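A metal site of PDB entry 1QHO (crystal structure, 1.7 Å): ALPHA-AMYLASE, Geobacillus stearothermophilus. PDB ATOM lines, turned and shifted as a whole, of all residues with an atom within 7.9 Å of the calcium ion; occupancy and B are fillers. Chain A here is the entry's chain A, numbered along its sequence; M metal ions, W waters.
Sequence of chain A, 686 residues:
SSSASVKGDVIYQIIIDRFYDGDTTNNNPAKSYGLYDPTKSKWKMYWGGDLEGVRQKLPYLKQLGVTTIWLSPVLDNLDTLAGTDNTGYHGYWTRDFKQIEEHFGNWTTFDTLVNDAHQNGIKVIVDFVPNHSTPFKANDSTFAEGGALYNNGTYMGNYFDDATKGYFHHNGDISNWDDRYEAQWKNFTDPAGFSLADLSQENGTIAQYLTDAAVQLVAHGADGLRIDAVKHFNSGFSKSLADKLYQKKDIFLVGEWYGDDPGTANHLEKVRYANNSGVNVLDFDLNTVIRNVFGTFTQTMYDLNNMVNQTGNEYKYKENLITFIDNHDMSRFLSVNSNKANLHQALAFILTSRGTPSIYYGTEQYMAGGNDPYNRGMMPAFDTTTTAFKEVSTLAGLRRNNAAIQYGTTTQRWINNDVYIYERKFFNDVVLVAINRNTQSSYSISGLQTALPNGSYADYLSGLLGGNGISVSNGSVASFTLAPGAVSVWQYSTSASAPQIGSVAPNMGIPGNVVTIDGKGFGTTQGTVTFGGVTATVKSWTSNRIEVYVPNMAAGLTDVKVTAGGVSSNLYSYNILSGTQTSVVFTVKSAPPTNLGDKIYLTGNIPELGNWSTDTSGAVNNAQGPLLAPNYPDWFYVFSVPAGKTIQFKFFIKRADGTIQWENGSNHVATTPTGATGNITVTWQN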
ATOM      1  N   PRO A  29      18.471 -25.221   5.040  1.00  0.00           N
ATOM      2  CA  PRO A  29      17.144 -24.806   5.475  1.00  0.00           C
ATOM      3  C   PRO A  29      17.152 -23.452   6.161  1.00  0.00           C
ATOM      4  O   PRO A  29      18.065 -23.136   6.921  1.00  0.00           O
ATOM      5  CB  PRO A  29      16.609 -25.874   6.450  1.00  0.00           C
ATOM      6  CG  PRO A  29      17.629 -26.977   6.320  1.00  0.00           C
ATOM      7  CD  PRO A  29      18.921 -26.415   5.759  1.00  0.00           C
ATOM      8  N   LYS A  31      15.567 -22.665   8.797  1.00  0.00           N
ATOM      9  CA  LYS A  31      15.654 -22.890  10.243  1.00  0.00           C
ATOM     10  C   LYS A  31      17.098 -22.809  10.754  1.00  0.00           C
ATOM     11  O   LYS A  31      17.314 -22.467  11.912  1.00  0.00           O
ATOM     12  CB  LYS A  31      15.064 -24.271  10.583  1.00  0.00           C
ATOM     13  CG  LYS A  31      15.105 -24.683  12.048  1.00  0.00           C
ATOM     14  CD  LYS A  31      14.199 -25.912  12.251  1.00  0.00           C
ATOM     15  CE  LYS A  31      14.268 -26.463  13.667  1.00  0.00           C
ATOM     16  NZ  LYS A  31      15.618 -27.004  13.984  1.00  0.00           N
ATOM     17  N   SER A  32      18.076 -23.260   9.979  1.00  0.00           N
ATOM     18  CA  SER A  32      19.478 -23.293  10.393  1.00  0.00           C
ATOM     19  C   SER A  32      20.345 -22.846   9.216  1.00  0.00           C
ATOM     20  O   SER A  32      21.324 -23.462   8.805  1.00  0.00           O
ATOM     21  CB  SER A  32      19.841 -24.726  10.787  1.00  0.00           C
ATOM     22  OG  SER A  32      19.441 -25.640   9.776  1.00  0.00           O
ATOM     23  N   LEU A  35      24.845 -22.966   7.498  1.00  0.00           N
ATOM     24  CA  LEU A  35      25.719 -24.005   8.051  1.00  0.00           C
ATOM     25  C   LEU A  35      26.152 -25.015   7.002  1.00  0.00           C
ATOM     26  O   LEU A  35      26.838 -25.993   7.323  1.00  0.00           O
ATOM     27  CB  LEU A  35      24.996 -24.768   9.172  1.00  0.00           C
ATOM     28  CG  LEU A  35      24.293 -23.927  10.234  1.00  0.00           C
ATOM     29  CD1 LEU A  35      23.657 -24.797  11.306  1.00  0.00           C
ATOM     30  CD2 LEU A  35      25.263 -22.917  10.868  1.00  0.00           C
ATOM     31  N   TYR A  46      28.024 -28.581   7.400  1.00  0.00           N
ATOM     32  CA  TYR A  46      27.219 -29.615   6.756  1.00  0.00           C
ATOM     33  C   TYR A  46      27.562 -29.690   5.267  1.00  0.00           C
ATOM     34  O   TYR A  46      27.613 -28.633   4.614  1.00  0.00           O
ATOM     35  CB  TYR A  46      25.718 -29.362   6.863  1.00  0.00           C
ATOM     36  CG  TYR A  46      25.037 -29.577   8.193  1.00  0.00           C
ATOM     37  CD1 TYR A  46      25.047 -28.582   9.159  1.00  0.00           C
ATOM     38  CD2 TYR A  46      24.346 -30.753   8.461  1.00  0.00           C
ATOM     39  CE1 TYR A  46      24.398 -28.745  10.375  1.00  0.00           C
ATOM     40  CE2 TYR A  46      23.687 -30.944   9.675  1.00  0.00           C
ATOM     41  CZ  TYR A  46      23.731 -29.927  10.609  1.00  0.00           C
ATOM     42  OH  TYR A  46      23.081 -30.078  11.813  1.00  0.00           O
ATOM     43  N   LEU A  75      18.750 -36.706  15.465  1.00  0.00           N
ATOM     44  CA  LEU A  75      17.858 -35.710  16.055  1.00  0.00           C
ATOM     45  C   LEU A  75      18.371 -34.288  15.893  1.00  0.00           C
ATOM     46  O   LEU A  75      19.527 -34.052  15.564  1.00  0.00           O
ATOM     47  CB  LEU A  75      17.560 -36.087  17.514  1.00  0.00           C
ATOM     48  CG  LEU A  75      16.955 -37.490  17.673  1.00  0.00           C
ATOM     49  CD1 LEU A  75      16.976 -37.979  19.115  1.00  0.00           C
ATOM     50  CD2 LEU A  75      15.512 -37.488  17.137  1.00  0.00           C
ATOM     51  N   ASP A  76      17.440 -33.349  15.982  1.00  0.00           N
ATOM     52  CA  ASP A  76      17.722 -31.934  15.687  1.00  0.00           C
ATOM     53  C   ASP A  76      18.931 -31.413  16.449  1.00  0.00           C
ATOM     54  O   ASP A  76      18.921 -31.347  17.672  1.00  0.00           O
ATOM     55  CB  ASP A  76      16.450 -31.160  16.028  1.00  0.00           C
ATOM     56  CG  ASP A  76      16.489 -29.690  15.710  1.00  0.00           C
ATOM     57  OD1 ASP A  76      17.388 -29.295  14.954  1.00  0.00           O
ATOM     58  OD2 ASP A  76      15.659 -28.886  16.165  1.00  0.00           O
ATOM     59  N   ASN A  77      19.951 -30.999  15.697  1.00  0.00           N
ATOM     60  CA  ASN A  77      21.166 -30.444  16.281  1.00  0.00           C
ATOM     61  C   ASN A  77      21.189 -28.921  16.234  1.00  0.00           C
ATOM     62  O   ASN A  77      20.413 -28.311  15.497  1.00  0.00           O
ATOM     63  CB  ASN A  77      22.405 -30.927  15.517  1.00  0.00           C
ATOM     64  CG  ASN A  77      22.978 -32.181  16.139  1.00  0.00           C
ATOM     65  OD1 ASN A  77      24.208 -32.255  16.285  1.00  0.00           O
ATOM     66  ND2 ASN A  77      22.142 -33.102  16.598  1.00  0.00           N
ATOM     67  N   LEU A  78      21.994 -28.292  17.043  1.00  0.00           N
ATOM     68  CA  LEU A  78      22.305 -26.869  17.026  1.00  0.00           C
ATOM     69  C   LEU A  78      22.034 -26.207  15.692  1.00  0.00           C
ATOM     70  O   LEU A  78      22.578 -26.610  14.651  1.00  0.00           O
ATOM     71  CB  LEU A  78      23.813 -26.768  17.355  1.00  0.00           C
ATOM     72  CG  LEU A  78      24.334 -25.311  17.443  1.00  0.00           C
ATOM     73  CD1 LEU A  78      23.735 -24.613  18.645  1.00  0.00           C
ATOM     74  CD2 LEU A  78      25.852 -25.337  17.528  1.00  0.00           C
ATOM     75  N   ASP A  79      21.229 -25.125  15.719  1.00  0.00           N
ATOM     76  CA  ASP A  79      20.866 -24.422  14.492  1.00  0.00           C
ATOM     77  C   ASP A  79      21.757 -23.233  14.157  1.00  0.00           C
ATOM     78  O   ASP A  79      21.455 -22.516  13.202  1.00  0.00           O
ATOM     79  CB  ASP A  79      19.421 -23.868  14.626  1.00  0.00           C
ATOM     80  CG  ASP A  79      18.374 -24.944  14.526  1.00  0.00           C
ATOM     81  OD1 ASP A  79      18.779 -26.034  14.078  1.00  0.00           O
ATOM     82  OD2 ASP A  79      17.188 -24.850  14.829  1.00  0.00           O
ATOM     83  N   THR A  80      22.810 -23.016  14.942  1.00  0.00           N
ATOM     84  CA  THR A  80      23.751 -21.928  14.721  1.00  0.00           C
ATOM     85  C   THR A  80      25.176 -22.493  14.587  1.00  0.00           C
ATOM     86  O   THR A  80      25.393 -23.694  14.747  1.00  0.00           O
ATOM     87  CB  THR A  80      23.814 -20.952  15.912  1.00  0.00           C
ATOM     88  OG1 THR A  80      24.439 -21.596  17.044  1.00  0.00           O
ATOM     89  CG2 THR A  80      22.460 -20.429  16.366  1.00  0.00           C
ATOM     90  N   GLY A  88      26.934 -28.656  13.984  1.00  0.00           N
ATOM     91  CA  GLY A  88      26.527 -29.996  14.430  1.00  0.00           C
ATOM     92  C   GLY A  88      26.291 -30.954  13.277  1.00  0.00           C
ATOM     93  O   GLY A  88      25.466 -31.880  13.415  1.00  0.00           O
ATOM     94  N   TRP A  93      25.332 -32.813  18.881  1.00  0.00           N
ATOM     95  CA  TRP A  93      24.980 -31.602  19.632  1.00  0.00           C
ATOM     96  C   TRP A  93      23.475 -31.346  19.493  1.00  0.00           C
ATOM     97  O   TRP A  93      23.029 -30.559  18.655  1.00  0.00           O
ATOM     98  CB  TRP A  93      25.776 -30.419  19.085  1.00  0.00           C
ATOM     99  CG  TRP A  93      27.276 -30.533  19.159  1.00  0.00           C
ATOM    100  CD1 TRP A  93      28.026 -31.367  19.933  1.00  0.00           C
ATOM    101  CD2 TRP A  93      28.205 -29.704  18.433  1.00  0.00           C
ATOM    102  NE1 TRP A  93      29.367 -31.136  19.716  1.00  0.00           N
ATOM    103  CE2 TRP A  93      29.487 -30.117  18.809  1.00  0.00           C
ATOM    104  CE3 TRP A  93      28.056 -28.677  17.500  1.00  0.00           C
ATOM    105  CZ2 TRP A  93      30.644 -29.539  18.279  1.00  0.00           C
ATOM    106  CZ3 TRP A  93      29.206 -28.094  16.984  1.00  0.00           C
ATOM    107  CH2 TRP A  93      30.482 -28.534  17.367  1.00  0.00           C
ATOM    108  N   ARG A  95      19.670 -30.240  20.091  1.00  0.00           N
ATOM    109  CA  ARG A  95      18.837 -29.202  20.691  1.00  0.00           C
ATOM    110  C   ARG A  95      17.406 -29.701  20.927  1.00  0.00           C
ATOM    111  O   ARG A  95      16.673 -29.046  21.661  1.00  0.00           O
ATOM    112  CB  ARG A  95      18.789 -27.948  19.830  1.00  0.00           C
ATOM    113  CG  ARG A  95      18.090 -28.130  18.481  1.00  0.00           C
ATOM    114  CD  ARG A  95      18.352 -26.932  17.577  1.00  0.00           C
ATOM    115  NE  ARG A  95      17.860 -25.635  18.000  1.00  0.00           N
ATOM    116  CZ  ARG A  95      16.598 -25.207  17.894  1.00  0.00           C
ATOM    117  NH1 ARG A  95      15.627 -25.987  17.450  1.00  0.00           N
ATOM    118  NH2 ARG A  95      16.334 -23.947  18.222  1.00  0.00           N
ATOM    119  N   ASP A  96      16.990 -30.760  20.229  1.00  0.00           N
ATOM    120  CA  ASP A  96      15.606 -31.224  20.380  1.00  0.00           C
ATOM    121  C   ASP A  96      15.603 -32.724  20.109  1.00  0.00           C
ATOM    122  O   ASP A  96      15.737 -33.142  18.959  1.00  0.00           O
ATOM    123  CB  ASP A  96      14.667 -30.495  19.424  1.00  0.00           C
ATOM    124  CG  ASP A  96      13.189 -30.756  19.668  1.00  0.00           C
ATOM    125  OD1 ASP A  96      12.827 -31.781  20.268  1.00  0.00           O
ATOM    126  OD2 ASP A  96      12.348 -29.917  19.232  1.00  0.00           O
ATOM    127  N   GLN A  99      12.664 -34.314  17.500  1.00  0.00           N
ATOM    128  CA  GLN A  99      12.547 -34.005  16.089  1.00  0.00           C
ATOM    129  C   GLN A  99      13.784 -34.428  15.293  1.00  0.00           C
ATOM    130  O   GLN A  99      14.897 -34.412  15.821  1.00  0.00           O
ATOM    131  CB  GLN A  99      12.381 -32.492  15.821  1.00  0.00           C
ATOM    132  CG  GLN A  99      11.044 -31.963  16.311  1.00  0.00           C
ATOM    133  CD  GLN A  99      10.447 -31.041  15.267  1.00  0.00           C
ATOM    134  OE1 GLN A  99      10.039 -31.507  14.190  1.00  0.00           O
ATOM    135  NE2 GLN A  99      10.412 -29.762  15.603  1.00  0.00           N
ATOM    136  N   ILE A 100      13.523 -34.820  14.053  1.00  0.00           N
ATOM    137  CA  ILE A 100      14.623 -35.170  13.167  1.00  0.00           C
ATOM    138  C   ILE A 100      15.352 -33.898  12.730  1.00  0.00           C
ATOM    139  O   ILE A 100      14.738 -32.845  12.497  1.00  0.00           O
ATOM    140  CB  ILE A 100      14.080 -35.896  11.928  1.00  0.00           C
ATOM    141  CG1 ILE A 100      13.394 -37.220  12.318  1.00  0.00           C
ATOM    142  CG2 ILE A 100      15.145 -36.166  10.866  1.00  0.00           C
ATOM    143  CD1 ILE A 100      14.308 -38.239  12.983  1.00  0.00           C
ATOM    144  N   GLU A 101      16.669 -33.997  12.599  1.00  0.00           N
ATOM    145  CA  GLU A 101      17.476 -32.881  12.091  1.00  0.00           C
ATOM    146  C   GLU A 101      16.998 -32.495  10.701  1.00  0.00           C
ATOM    147  O   GLU A 101      16.965 -33.326   9.799  1.00  0.00           O
ATOM    148  CB  GLU A 101      18.949 -33.297  12.080  1.00  0.00           C
ATOM    149  CG  GLU A 101      19.869 -32.424  11.227  1.00  0.00           C
ATOM    150  CD  GLU A 101      19.749 -30.959  11.631  1.00  0.00           C
ATOM    151  OE1 GLU A 101      19.737 -30.747  12.867  1.00  0.00           O
ATOM    152  OE2 GLU A 101      19.696 -30.081  10.753  1.00  0.00           O
ATOM    153  N   GLU A 102      16.692 -31.203  10.526  1.00  0.00           N
ATOM    154  CA  GLU A 102      16.119 -30.733   9.260  1.00  0.00           C
ATOM    155  C   GLU A 102      17.040 -30.849   8.065  1.00  0.00           C
ATOM    156  O   GLU A 102      16.556 -31.042   6.938  1.00  0.00           O
ATOM    157  CB  GLU A 102      15.571 -29.298   9.396  1.00  0.00           C
ATOM    158  CG  GLU A 102      16.628 -28.210   9.547  1.00  0.00           C
ATOM    159  CD  GLU A 102      17.188 -28.107  10.932  1.00  0.00           C
ATOM    160  OE1 GLU A 102      16.719 -28.760  11.888  1.00  0.00           O
ATOM    161  OE2 GLU A 102      18.161 -27.318  11.103  1.00  0.00           O
ATOM    162  N   HIS A 103      18.373 -30.812   8.233  1.00  0.00           N
ATOM    163  CA  HIS A 103      19.273 -31.086   7.130  1.00  0.00           C
ATOM    164  C   HIS A 103      19.150 -32.525   6.651  1.00  0.00           C
ATOM    165  O   HIS A 103      19.508 -32.812   5.503  1.00  0.00           O
ATOM    166  CB  HIS A 103      20.747 -30.864   7.548  1.00  0.00           C
ATOM    167  CG  HIS A 103      21.145 -29.432   7.666  1.00  0.00           C
ATOM    168  ND1 HIS A 103      20.933 -28.691   8.816  1.00  0.00           N
ATOM    169  CD2 HIS A 103      21.735 -28.607   6.782  1.00  0.00           C
ATOM    170  CE1 HIS A 103      21.393 -27.453   8.619  1.00  0.00           C
ATOM    171  NE2 HIS A 103      21.885 -27.385   7.395  1.00  0.00           N
ATOM    172  N   PHE A 104      18.688 -33.438   7.508  1.00  0.00           N
ATOM    173  CA  PHE A 104      18.618 -34.850   7.145  1.00  0.00           C
ATOM    174  C   PHE A 104      17.255 -35.336   6.668  1.00  0.00           C
ATOM    175  O   PHE A 104      17.219 -36.364   5.980  1.00  0.00           O
ATOM    176  CB  PHE A 104      19.101 -35.712   8.325  1.00  0.00           C
ATOM    177  CG  PHE A 104      20.497 -35.438   8.818  1.00  0.00           C
ATOM    178  CD1 PHE A 104      21.435 -34.749   8.075  1.00  0.00           C
ATOM    179  CD2 PHE A 104      20.886 -35.935  10.056  1.00  0.00           C
ATOM    180  CE1 PHE A 104      22.718 -34.511   8.540  1.00  0.00           C
ATOM    181  CE2 PHE A 104      22.162 -35.712  10.538  1.00  0.00           C
ATOM    182  CZ  PHE A 104      23.090 -34.994   9.785  1.00  0.00           C
ATOM    183  N   GLU A 145      23.735 -21.547  21.061  1.00  0.00           N
ATOM    184  CA  GLU A 145      22.381 -21.364  21.591  1.00  0.00           C
ATOM    185  C   GLU A 145      22.367 -21.400  23.103  1.00  0.00           C
ATOM    186  O   GLU A 145      21.340 -21.681  23.758  1.00  0.00           O
ATOM    187  CB  GLU A 145      21.415 -22.410  20.995  1.00  0.00           C
ATOM    188  CG  GLU A 145      21.192 -22.196  19.505  1.00  0.00           C
ATOM    189  CD  GLU A 145      20.419 -23.310  18.812  1.00  0.00           C
ATOM    190  OE1 GLU A 145      19.911 -24.235  19.446  1.00  0.00           O
ATOM    191  OE2 GLU A 145      20.348 -23.281  17.569  1.00  0.00           O
HETATM  192 CA    CA M   1      19.036 -28.371  13.349  1.00  0.00          CA
HETATM  193  O   HOH W   1      21.401 -27.882  12.470  1.00  0.00           O
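The calcium ion is bound by OD1 of Asp 79 (2.5 Å), OD1 of Asp 76 (2.5 Å), OE1 of Glu 101 (2.5 Å), O of Asn 77 (2.6 Å), water W1 (2.6 Å), OE2 of Glu 102 (2.6 Å) and OE1 of Glu 102 (2.8 Å). The calcium ion has seven donor atoms within binding distance.
OD2 of Asp 79 is in salt-bridge range of NH1 of Arg 95 (3.3 Å). NZ of Lys 31 is in salt-bridge range of OD2 of Asp 76, at 2.9 Å. The backbone NH (N) of Asp 76 sits at hydrogen-bond distance from the backbone carbonyl oxygen (O) of Gln 99. OE2 of Glu 101 lies within hydrogen-bond range of ND1 of His 103, 2.7 Å away. The side-chain amide nitrogen (ND2) of Asn 77 lies within hydrogen-bond range of the backbone carbonyl oxygen (O) of Leu 75, 3.0 Å away. The side-chain amide oxygen (OD1) of Asn 77 lies close to the backbone carbonyl oxygen (O) of Gly 88 (3.2 Å). The side-chain carboxylate of Glu 102 lies close to the side-chain amino group of Lys 31 (2.9 Å). OG of Ser 32 lies close to OE2 of Glu 102 (2.5 Å).
Lys 31 touches the calcium ion (NZ to CA, 3.7 Å). Six residues have an atom within 4 Å of the calcium ion: Lys 31, Asp 76, Asn 77, Asp 79, Glu 101 and Glu 102.
Water W1 lies within hydrogen-bond range of the backbone carbonyl oxygen (O) of Leu 78 (2.8 Å), the side-chain hydroxyl (OH) of Tyr 46 (2.8 Å) and the side-chain carboxylate (OE2) of Glu 101 (3.3 Å).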
